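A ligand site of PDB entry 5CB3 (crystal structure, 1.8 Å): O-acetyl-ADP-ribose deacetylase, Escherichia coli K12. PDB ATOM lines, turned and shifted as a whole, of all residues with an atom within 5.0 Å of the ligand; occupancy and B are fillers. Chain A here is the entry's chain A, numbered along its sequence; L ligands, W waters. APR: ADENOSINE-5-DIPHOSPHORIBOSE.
The side-chain carboxylate (OD2) of Asp 41 sits at hydrogen-bond distance from an oxygen (O2D) of the ligand (2.6 Å). ND2 of Asn 31 is in hydrogen-bond range of O2D of the ligand (2.8 Å). The backbone NH (N) of Gly 130 is in hydrogen-bond range of an oxygen (O2B) of the ligand (2.8 Å). An oxygen (O1B) of the ligand is in hydrogen-bond range of the backbone NH (N) of Ser 128, at 2.8 Å. O1A of the ligand lies within hydrogen-bond range of N of Val 131, 2.8 Å away. An oxygen (O2A) of the ligand is in hydrogen-bond range of the backbone NH of Val 40, 2.8 Å away. An oxygen (O1D) of the ligand sits at hydrogen-bond distance from the backbone NH (N) of Gly 39 (2.9 Å). A nitrogen (N6) of the ligand is in hydrogen-bond range of the side-chain carboxylate (OD1) of Asp 17 (2.9 Å). N of Ile 18 sits at hydrogen-bond distance from N1 of the ligand (3.0 Å). The backbone NH (N) of Thr 129 is in hydrogen-bond range of an oxygen (O2B) of the ligand, at 3.4 Å. An oxygen (O3') of the ligand sits at hydrogen-bond distance from the side-chain hydroxyl (OG1) of Thr 129 (3.1 Å). An oxygen (O2B) of the ligand lies within hydrogen-bond range of the backbone NH (N) of Tyr 132 (3.1 Å). The backbone NH (N) of Gly 38 is in hydrogen-bond range of an oxygen (O1D) of the ligand, 3.1 Å away.
The side-chain carboxylate of Asp 41 sits at hydrogen-bond distance from the backbone NH of Gly 37 (3.4 Å). ND2 of Asn 31 is in hydrogen-bond range of O of Gly 36 (2.8 Å). The backbone carbonyl oxygen (O) of Ser 128 is in hydrogen-bond range of the backbone NH (N) of Gly 133 (3.1 Å). OD1 of Asp 17 sits at hydrogen-bond distance from OG1 of Thr 19 (2.7 Å). The side-chain hydroxyl (OG1) of Thr 129 lies within hydrogen-bond range of the backbone carbonyl oxygen (O) of Ala 126 (2.7 Å). O of Gly 37 lies close to N of Gly 42 (3.2 Å).
Merely in contact with the ligand: Ala 126, Tyr 165, Gly 37, Gly 36, Ala 29, Gly 16, Ala 30, Ala 43 and Ile 127. Hydrophobic or aromatic side chains within 4 Å of the ligand: Ile 18, Ala 29, Val 40, Ala 43, Ala 126, Val 131, Tyr 132 and Tyr 165. Of the 28 residues printed, 21 come within 4 Å of the ligand.
Water W6 lies within hydrogen-bond range of an oxygen (O1D) of the ligand, the backbone carbonyl oxygen of Ala 29, the backbone NH of Asp 41 and the backbone NH of Val 40. Water W7 lies within hydrogen-bond range of a nitrogen (N6) of the ligand and the side-chain hydroxyl of Tyr 165. Water W5 lies within hydrogen-bond range of O4D of the ligand (2.8 Å) and N of Gly 39 (2.9 Å). Water W9 lies within hydrogen-bond range of O of Val 163, N3 of the ligand and N of Ala 126. Water W1 lies within hydrogen-bond range of the backbone carbonyl oxygen (O) of Ala 30 (2.9 Å) and an oxygen (O1B) of the ligand (2.9 Å). Water W4 lies within hydrogen-bond range of the guanidinium group of Arg 136 (2.7 Å), the backbone carbonyl oxygen of Thr 129 (3.0 Å) and an oxygen (O3') of the ligand (3.0 Å).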
ATOM      1  N   GLY A  16      14.407  19.556 -23.262  1.00  0.00           N
ATOM      2  CA  GLY A  16      14.030  18.178 -23.024  1.00  0.00           C
ATOM      3  C   GLY A  16      13.200  17.947 -21.776  1.00  0.00           C
ATOM      4  O   GLY A  16      12.609  18.864 -21.206  1.00  0.00           O
ATOM      5  N   ASP A  17      13.190  16.688 -21.373  1.00  0.00           N
ATOM      6  CA  ASP A  17      12.444  16.172 -20.242  1.00  0.00           C
ATOM      7  C   ASP A  17      13.311  16.278 -18.983  1.00  0.00           C
ATOM      8  O   ASP A  17      14.385  15.668 -18.926  1.00  0.00           O
ATOM      9  CB  ASP A  17      12.152  14.712 -20.568  1.00  0.00           C
ATOM     10  CG  ASP A  17      11.323  14.016 -19.526  1.00  0.00           C
ATOM     11  OD1 ASP A  17      11.130  14.542 -18.403  1.00  0.00           O
ATOM     12  OD2 ASP A  17      10.840  12.909 -19.845  1.00  0.00           O
ATOM     13  N   ILE A  18      12.853  17.017 -17.980  1.00  0.00           N
ATOM     14  CA  ILE A  18      13.615  17.189 -16.740  1.00  0.00           C
ATOM     15  C   ILE A  18      13.892  15.865 -16.010  1.00  0.00           C
ATOM     16  O   ILE A  18      14.884  15.751 -15.293  1.00  0.00           O
ATOM     17  CB  ILE A  18      12.930  18.215 -15.784  1.00  0.00           C
ATOM     18  CG1 ILE A  18      13.917  18.743 -14.734  1.00  0.00           C
ATOM     19  CG2 ILE A  18      11.667  17.611 -15.159  1.00  0.00           C
ATOM     20  CD1 ILE A  18      13.364  19.903 -13.928  1.00  0.00           C
ATOM     21  N   THR A  19      13.014  14.871 -16.212  1.00  0.00           N
ATOM     22  CA  THR A  19      13.158  13.576 -15.524  1.00  0.00           C
ATOM     23  C   THR A  19      14.362  12.749 -16.004  1.00  0.00           C
ATOM     24  O   THR A  19      14.744  11.789 -15.349  1.00  0.00           O
ATOM     25  CB  THR A  19      11.870  12.710 -15.610  1.00  0.00           C
ATOM     26  OG1 THR A  19      11.610  12.296 -16.959  1.00  0.00           O
ATOM     27  CG2 THR A  19      10.656  13.458 -15.059  1.00  0.00           C
ATOM     28  N   ALA A  29       7.288  21.488 -10.138  1.00  0.00           N
ATOM     29  CA  ALA A  29       6.244  22.496 -10.121  1.00  0.00           C
ATOM     30  C   ALA A  29       4.960  21.841  -9.634  1.00  0.00           C
ATOM     31  O   ALA A  29       4.134  21.352 -10.404  1.00  0.00           O
ATOM     32  CB  ALA A  29       6.058  23.114 -11.497  1.00  0.00           C
ATOM     33  N   ALA A  30       4.828  21.820  -8.307  1.00  0.00           N
ATOM     34  CA  ALA A  30       3.815  21.042  -7.626  1.00  0.00           C
ATOM     35  C   ALA A  30       2.537  21.838  -7.379  1.00  0.00           C
ATOM     36  O   ALA A  30       2.382  22.959  -7.858  1.00  0.00           O
ATOM     37  CB  ALA A  30       4.399  20.556  -6.300  1.00  0.00           C
ATOM     38  N   ASN A  31       1.618  21.220  -6.646  1.00  0.00           N
ATOM     39  CA  ASN A  31       0.472  21.909  -6.069  1.00  0.00           C
ATOM     40  C   ASN A  31       0.537  21.695  -4.555  1.00  0.00           C
ATOM     41  O   ASN A  31       1.298  20.840  -4.094  1.00  0.00           O
ATOM     42  CB  ASN A  31      -0.841  21.384  -6.651  1.00  0.00           C
ATOM     43  CG  ASN A  31      -1.134  19.950  -6.236  1.00  0.00           C
ATOM     44  OD1 ASN A  31      -1.662  19.706  -5.146  1.00  0.00           O
ATOM     45  ND2 ASN A  31      -0.790  18.990  -7.092  1.00  0.00           N
ATOM     46  N   GLY A  36       0.903  15.131  -6.363  1.00  0.00           N
ATOM     47  CA  GLY A  36       1.062  14.979  -7.808  1.00  0.00           C
ATOM     48  C   GLY A  36       0.027  15.737  -8.626  1.00  0.00           C
ATOM     49  O   GLY A  36      -0.839  16.409  -8.082  1.00  0.00           O
ATOM     50  N   GLY A  37       0.143  15.617  -9.946  1.00  0.00           N
ATOM     51  CA  GLY A  37      -0.781  16.284 -10.862  1.00  0.00           C
ATOM     52  C   GLY A  37      -0.468  15.898 -12.295  1.00  0.00           C
ATOM     53  O   GLY A  37       0.113  14.850 -12.542  1.00  0.00           O
ATOM     54  N   GLY A  38      -0.866  16.742 -13.246  1.00  0.00           N
ATOM     55  CA  GLY A  38      -0.834  16.333 -14.656  1.00  0.00           C
ATOM     56  C   GLY A  38       0.280  16.796 -15.561  1.00  0.00           C
ATOM     57  O   GLY A  38       0.394  16.308 -16.685  1.00  0.00           O
ATOM     58  N   GLY A  39       1.134  17.708 -15.110  1.00  0.00           N
ATOM     59  CA  GLY A  39       2.175  18.256 -15.998  1.00  0.00           C
ATOM     60  C   GLY A  39       3.524  17.653 -15.664  1.00  0.00           C
ATOM     61  O   GLY A  39       3.667  16.434 -15.635  1.00  0.00           O
ATOM     62  N   VAL A  40       4.503  18.516 -15.418  1.00  0.00           N
ATOM     63  CA  VAL A  40       5.839  18.051 -15.020  1.00  0.00           C
ATOM     64  C   VAL A  40       5.752  17.325 -13.664  1.00  0.00           C
ATOM     65  O   VAL A  40       6.522  16.396 -13.418  1.00  0.00           O
ATOM     66  CB  VAL A  40       6.883  19.206 -15.014  1.00  0.00           C
ATOM     67  CG1 VAL A  40       6.613  20.224 -13.919  1.00  0.00           C
ATOM     68  CG2 VAL A  40       8.295  18.647 -14.898  1.00  0.00           C
ATOM     69  N   ASP A  41       4.802  17.726 -12.822  1.00  0.00           N
ATOM     70  CA  ASP A  41       4.520  17.066 -11.535  1.00  0.00           C
ATOM     71  C   ASP A  41       4.244  15.579 -11.763  1.00  0.00           C
ATOM     72  O   ASP A  41       4.909  14.708 -11.186  1.00  0.00           O
ATOM     73  CB  ASP A  41       3.327  17.751 -10.860  1.00  0.00           C
ATOM     74  CG  ASP A  41       3.184  17.430  -9.371  1.00  0.00           C
ATOM     75  OD1 ASP A  41       3.997  16.669  -8.802  1.00  0.00           O
ATOM     76  OD2 ASP A  41       2.243  17.979  -8.776  1.00  0.00           O
ATOM     77  N   GLY A  42       3.276  15.287 -12.631  1.00  0.00           N
ATOM     78  CA  GLY A  42       2.953  13.893 -12.958  1.00  0.00           C
ATOM     79  C   GLY A  42       4.110  13.144 -13.585  1.00  0.00           C
ATOM     80  O   GLY A  42       4.331  11.978 -13.269  1.00  0.00           O
ATOM     81  N   ALA A  43       4.861  13.822 -14.448  1.00  0.00           N
ATOM     82  CA  ALA A  43       6.019  13.224 -15.094  1.00  0.00           C
ATOM     83  C   ALA A  43       7.077  12.835 -14.070  1.00  0.00           C
ATOM     84  O   ALA A  43       7.674  11.776 -14.171  1.00  0.00           O
ATOM     85  CB  ALA A  43       6.598  14.177 -16.126  1.00  0.00           C
ATOM     86  N   PRO A 125      12.094  23.373 -14.034  1.00  0.00           N
ATOM     87  CA  PRO A 125      11.149  23.528 -15.117  1.00  0.00           C
ATOM     88  C   PRO A 125      10.612  24.956 -15.138  1.00  0.00           C
ATOM     89  O   PRO A 125      10.930  25.740 -14.237  1.00  0.00           O
ATOM     90  CB  PRO A 125      10.042  22.571 -14.713  1.00  0.00           C
ATOM     91  CG  PRO A 125      10.007  22.665 -13.225  1.00  0.00           C
ATOM     92  CD  PRO A 125      11.418  22.978 -12.784  1.00  0.00           C
ATOM     93  N   ALA A 126       9.797  25.282 -16.130  1.00  0.00           N
ATOM     94  CA  ALA A 126       9.230  26.620 -16.249  1.00  0.00           C
ATOM     95  C   ALA A 126       8.000  26.745 -15.345  1.00  0.00           C
ATOM     96  O   ALA A 126       6.862  26.693 -15.815  1.00  0.00           O
ATOM     97  CB  ALA A 126       8.879  26.918 -17.703  1.00  0.00           C
ATOM     98  N   ILE A 127       8.254  26.917 -14.049  1.00  0.00           N
ATOM     99  CA  ILE A 127       7.210  26.922 -13.009  1.00  0.00           C
ATOM    100  C   ILE A 127       6.074  27.886 -13.364  1.00  0.00           C
ATOM    101  O   ILE A 127       6.328  29.024 -13.793  1.00  0.00           O
ATOM    102  CB  ILE A 127       7.816  27.307 -11.629  1.00  0.00           C
ATOM    103  CG1 ILE A 127       8.803  26.235 -11.162  1.00  0.00           C
ATOM    104  CG2 ILE A 127       6.732  27.491 -10.569  1.00  0.00           C
ATOM    105  CD1 ILE A 127       9.683  26.709 -10.017  1.00  0.00           C
ATOM    106  N   SER A 128       4.834  27.416 -13.210  1.00  0.00           N
ATOM    107  CA  SER A 128       3.617  28.229 -13.381  1.00  0.00           C
ATOM    108  C   SER A 128       3.241  28.539 -14.827  1.00  0.00           C
ATOM    109  O   SER A 128       2.212  29.211 -15.057  1.00  0.00           O
ATOM    110  CB  SER A 128       3.703  29.558 -12.613  1.00  0.00           C
ATOM    111  OG  SER A 128       3.586  29.387 -11.220  1.00  0.00           O
ATOM    112  N   THR A 129       4.021  28.106 -15.812  1.00  0.00           N
ATOM    113  CA  THR A 129       3.728  28.501 -17.195  1.00  0.00           C
ATOM    114  C   THR A 129       2.890  27.488 -17.950  1.00  0.00           C
ATOM    115  O   THR A 129       2.579  27.707 -19.117  1.00  0.00           O
ATOM    116  CB  THR A 129       4.995  28.761 -18.037  1.00  0.00           C
ATOM    117  OG1 THR A 129       5.735  27.542 -18.175  1.00  0.00           O
ATOM    118  CG2 THR A 129       5.847  29.832 -17.415  1.00  0.00           C
ATOM    119  N   GLY A 130       2.549  26.388 -17.308  1.00  0.00           N
ATOM    120  CA  GLY A 130       1.717  25.380 -17.922  1.00  0.00           C
ATOM    121  C   GLY A 130       0.286  25.630 -17.520  1.00  0.00           C
ATOM    122  O   GLY A 130      -0.309  26.637 -17.901  1.00  0.00           O
ATOM    123  N   VAL A 131      -0.269  24.731 -16.713  1.00  0.00           N
ATOM    124  CA  VAL A 131      -1.676  24.868 -16.328  1.00  0.00           C
ATOM    125  C   VAL A 131      -1.937  26.105 -15.447  1.00  0.00           C
ATOM    126  O   VAL A 131      -3.064  26.587 -15.402  1.00  0.00           O
ATOM    127  CB  VAL A 131      -2.264  23.605 -15.664  1.00  0.00           C
ATOM    128  CG1 VAL A 131      -1.931  22.343 -16.461  1.00  0.00           C
ATOM    129  CG2 VAL A 131      -1.813  23.457 -14.229  1.00  0.00           C
ATOM    130  N   TYR A 132      -0.908  26.612 -14.754  1.00  0.00           N
ATOM    131  CA  TYR A 132      -1.076  27.803 -13.920  1.00  0.00           C
ATOM    132  C   TYR A 132      -1.075  29.101 -14.735  1.00  0.00           C
ATOM    133  O   TYR A 132      -1.415  30.160 -14.217  1.00  0.00           O
ATOM    134  CB  TYR A 132      -0.028  27.824 -12.788  1.00  0.00           C
ATOM    135  CG  TYR A 132      -0.385  26.940 -11.593  1.00  0.00           C
ATOM    136  CD1 TYR A 132      -1.497  26.097 -11.635  1.00  0.00           C
ATOM    137  CD2 TYR A 132       0.401  26.932 -10.448  1.00  0.00           C
ATOM    138  CE1 TYR A 132      -1.824  25.287 -10.552  1.00  0.00           C
ATOM    139  CE2 TYR A 132       0.086  26.130  -9.365  1.00  0.00           C
ATOM    140  CZ  TYR A 132      -1.029  25.305  -9.420  1.00  0.00           C
ATOM    141  OH  TYR A 132      -1.346  24.507  -8.354  1.00  0.00           O
ATOM    142  N   GLY A 133      -0.683  29.016 -16.008  1.00  0.00           N
ATOM    143  CA  GLY A 133      -0.990  30.054 -17.006  1.00  0.00           C
ATOM    144  C   GLY A 133      -0.227  31.366 -16.915  1.00  0.00           C
ATOM    145  O   GLY A 133      -0.708  32.399 -17.375  1.00  0.00           O
ATOM    146  N   ARG A 136       4.561  33.592 -20.448  1.00  0.00           N
ATOM    147  CA  ARG A 136       5.852  32.917 -20.519  1.00  0.00           C
ATOM    148  C   ARG A 136       7.067  33.851 -20.463  1.00  0.00           C
ATOM    149  O   ARG A 136       8.026  33.583 -19.747  1.00  0.00           O
ATOM    150  CB  ARG A 136       5.932  32.051 -21.759  1.00  0.00           C
ATOM    151  CG  ARG A 136       5.083  30.803 -21.702  1.00  0.00           C
ATOM    152  CD  ARG A 136       5.204  30.076 -23.026  1.00  0.00           C
ATOM    153  NE  ARG A 136       5.301  28.645 -22.834  1.00  0.00           N
ATOM    154  CZ  ARG A 136       5.988  27.800 -23.595  1.00  0.00           C
ATOM    155  NH1 ARG A 136       6.698  28.210 -24.658  1.00  0.00           N
ATOM    156  NH2 ARG A 136       5.968  26.514 -23.283  1.00  0.00           N
ATOM    157  N   VAL A 163      15.380  23.856 -17.644  1.00  0.00           N
ATOM    158  CA  VAL A 163      14.900  22.818 -18.545  1.00  0.00           C
ATOM    159  C   VAL A 163      13.607  23.306 -19.187  1.00  0.00           C
ATOM    160  O   VAL A 163      12.617  23.576 -18.508  1.00  0.00           O
ATOM    161  CB  VAL A 163      14.707  21.469 -17.857  1.00  0.00           C
ATOM    162  CG1 VAL A 163      14.284  20.415 -18.863  1.00  0.00           C
ATOM    163  CG2 VAL A 163      16.003  21.059 -17.176  1.00  0.00           C
ATOM    164  N   TYR A 165      10.701  22.652 -22.148  1.00  0.00           N
ATOM    165  CA  TYR A 165      10.044  21.474 -22.712  1.00  0.00           C
ATOM    166  C   TYR A 165       9.734  21.658 -24.180  1.00  0.00           C
ATOM    167  O   TYR A 165       9.362  20.705 -24.857  1.00  0.00           O
ATOM    168  CB  TYR A 165       8.757  21.176 -21.944  1.00  0.00           C
ATOM    169  CG  TYR A 165       8.279  19.742 -22.062  1.00  0.00           C
ATOM    170  CD1 TYR A 165       9.137  18.677 -21.802  1.00  0.00           C
ATOM    171  CD2 TYR A 165       6.958  19.459 -22.401  1.00  0.00           C
ATOM    172  CE1 TYR A 165       8.692  17.368 -21.897  1.00  0.00           C
ATOM    173  CE2 TYR A 165       6.512  18.151 -22.496  1.00  0.00           C
ATOM    174  CZ  TYR A 165       7.378  17.114 -22.235  1.00  0.00           C
ATOM    175  OH  TYR A 165       6.928  15.814 -22.333  1.00  0.00           O
ATOM    176  N   ASN A 169      10.366  28.056 -25.487  1.00  0.00           N
ATOM    177  CA  ASN A 169      10.711  28.451 -24.127  1.00  0.00           C
ATOM    178  C   ASN A 169      12.228  28.496 -24.027  1.00  0.00           C
ATOM    179  O   ASN A 169      12.790  29.377 -23.389  1.00  0.00           O
ATOM    180  CB  ASN A 169      10.118  27.495 -23.082  1.00  0.00           C
ATOM    181  CG  ASN A 169       9.396  28.224 -21.946  1.00  0.00           C
ATOM    182  OD1 ASN A 169       9.196  29.441 -21.991  1.00  0.00           O
ATOM    183  ND2 ASN A 169       8.990  27.464 -20.933  1.00  0.00           N
HETATM  184  N1  APR L   1      10.199  18.246 -18.388  1.00  0.00           N
HETATM  185  C2  APR L   1      10.351  19.591 -18.385  1.00  0.00           C
HETATM  186  N3  APR L   1       9.316  20.444 -18.472  1.00  0.00           N
HETATM  187  C4  APR L   1       8.043  19.985 -18.570  1.00  0.00           C
HETATM  188  C5  APR L   1       7.797  18.547 -18.577  1.00  0.00           C
HETATM  189  C6  APR L   1       8.981  17.665 -18.474  1.00  0.00           C
HETATM  190  N6  APR L   1       8.819  16.323 -18.487  1.00  0.00           N
HETATM  191  N7  APR L   1       6.466  18.382 -18.676  1.00  0.00           N
HETATM  192  C8  APR L   1       5.893  19.606 -18.728  1.00  0.00           C
HETATM  193  N9  APR L   1       6.851  20.558 -18.672  1.00  0.00           N
HETATM  194  C1' APR L   1       6.694  22.025 -18.668  1.00  0.00           C
HETATM  195  C2' APR L   1       5.374  22.576 -19.190  1.00  0.00           C
HETATM  196  O2' APR L   1       5.310  22.481 -20.619  1.00  0.00           O
HETATM  197  C3' APR L   1       5.482  23.990 -18.657  1.00  0.00           C
HETATM  198  O3' APR L   1       6.294  24.800 -19.525  1.00  0.00           O
HETATM  199  O4' APR L   1       6.773  22.511 -17.329  1.00  0.00           O
HETATM  200  C4' APR L   1       6.169  23.804 -17.308  1.00  0.00           C
HETATM  201  C5' APR L   1       5.197  23.925 -16.133  1.00  0.00           C
HETATM  202  O5' APR L   1       3.926  23.402 -16.510  1.00  0.00           O
HETATM  203  PA  APR L   1       3.011  22.575 -15.489  1.00  0.00           P
HETATM  204  O1A APR L   1       1.587  22.728 -16.000  1.00  0.00           O
HETATM  205  O2A APR L   1       3.653  21.220 -15.339  1.00  0.00           O
HETATM  206  O3A APR L   1       3.167  23.320 -14.062  1.00  0.00           O
HETATM  207  PB  APR L   1       2.429  24.666 -13.550  1.00  0.00           P
HETATM  208  O1B APR L   1       3.294  25.206 -12.432  1.00  0.00           O
HETATM  209  O2B APR L   1       2.031  25.606 -14.668  1.00  0.00           O
HETATM  210  O5D APR L   1       1.067  24.117 -12.911  1.00  0.00           O
HETATM  211  C5D APR L   1       1.117  23.325 -11.723  1.00  0.00           C
HETATM  212  O4D APR L   1       0.000  21.403 -12.649  1.00  0.00           O
HETATM  213  O1D APR L   1       0.962  19.235 -12.709  1.00  0.00           O
HETATM  214  C1D APR L   1       0.072  20.117 -12.019  1.00  0.00           C
HETATM  215  O2D APR L   1       0.192  19.374  -9.671  1.00  0.00           O
HETATM  216  C2D APR L   1       0.566  20.386 -10.609  1.00  0.00           C
HETATM  217  O3D APR L   1      -1.487  21.402 -10.000  1.00  0.00           O
HETATM  218  C3D APR L   1      -0.129  21.683 -10.330  1.00  0.00           C
HETATM  219  C4D APR L   1      -0.090  22.421 -11.644  1.00  0.00           C
HETATM  220  O   HOH W   1       3.694  24.931  -9.524  1.00  0.00           O
HETATM  221  O   HOH W   2       0.874  21.353 -18.319  1.00  0.00           O
HETATM  222  O   HOH W   3       2.743  19.814 -19.798  1.00  0.00           O
HETATM  223  O   HOH W   4       4.302  26.350 -21.128  1.00  0.00           O
HETATM  224  O   HOH W   5      -0.045  20.339 -15.232  1.00  0.00           O
HETATM  225  O   HOH W   6       3.399  20.280 -12.757  1.00  0.00           O
HETATM  226  O   HOH W   7       7.068  14.621 -19.785  1.00  0.00           O
HETATM  227  O   HOH W   8       9.053  24.567 -20.901  1.00  0.00           O
HETATM  228  O   HOH W   9       9.927  23.299 -18.279  1.00  0.00           O
HETATM  229  O   HOH W  10       4.743  16.253 -19.319  1.00  0.00           O
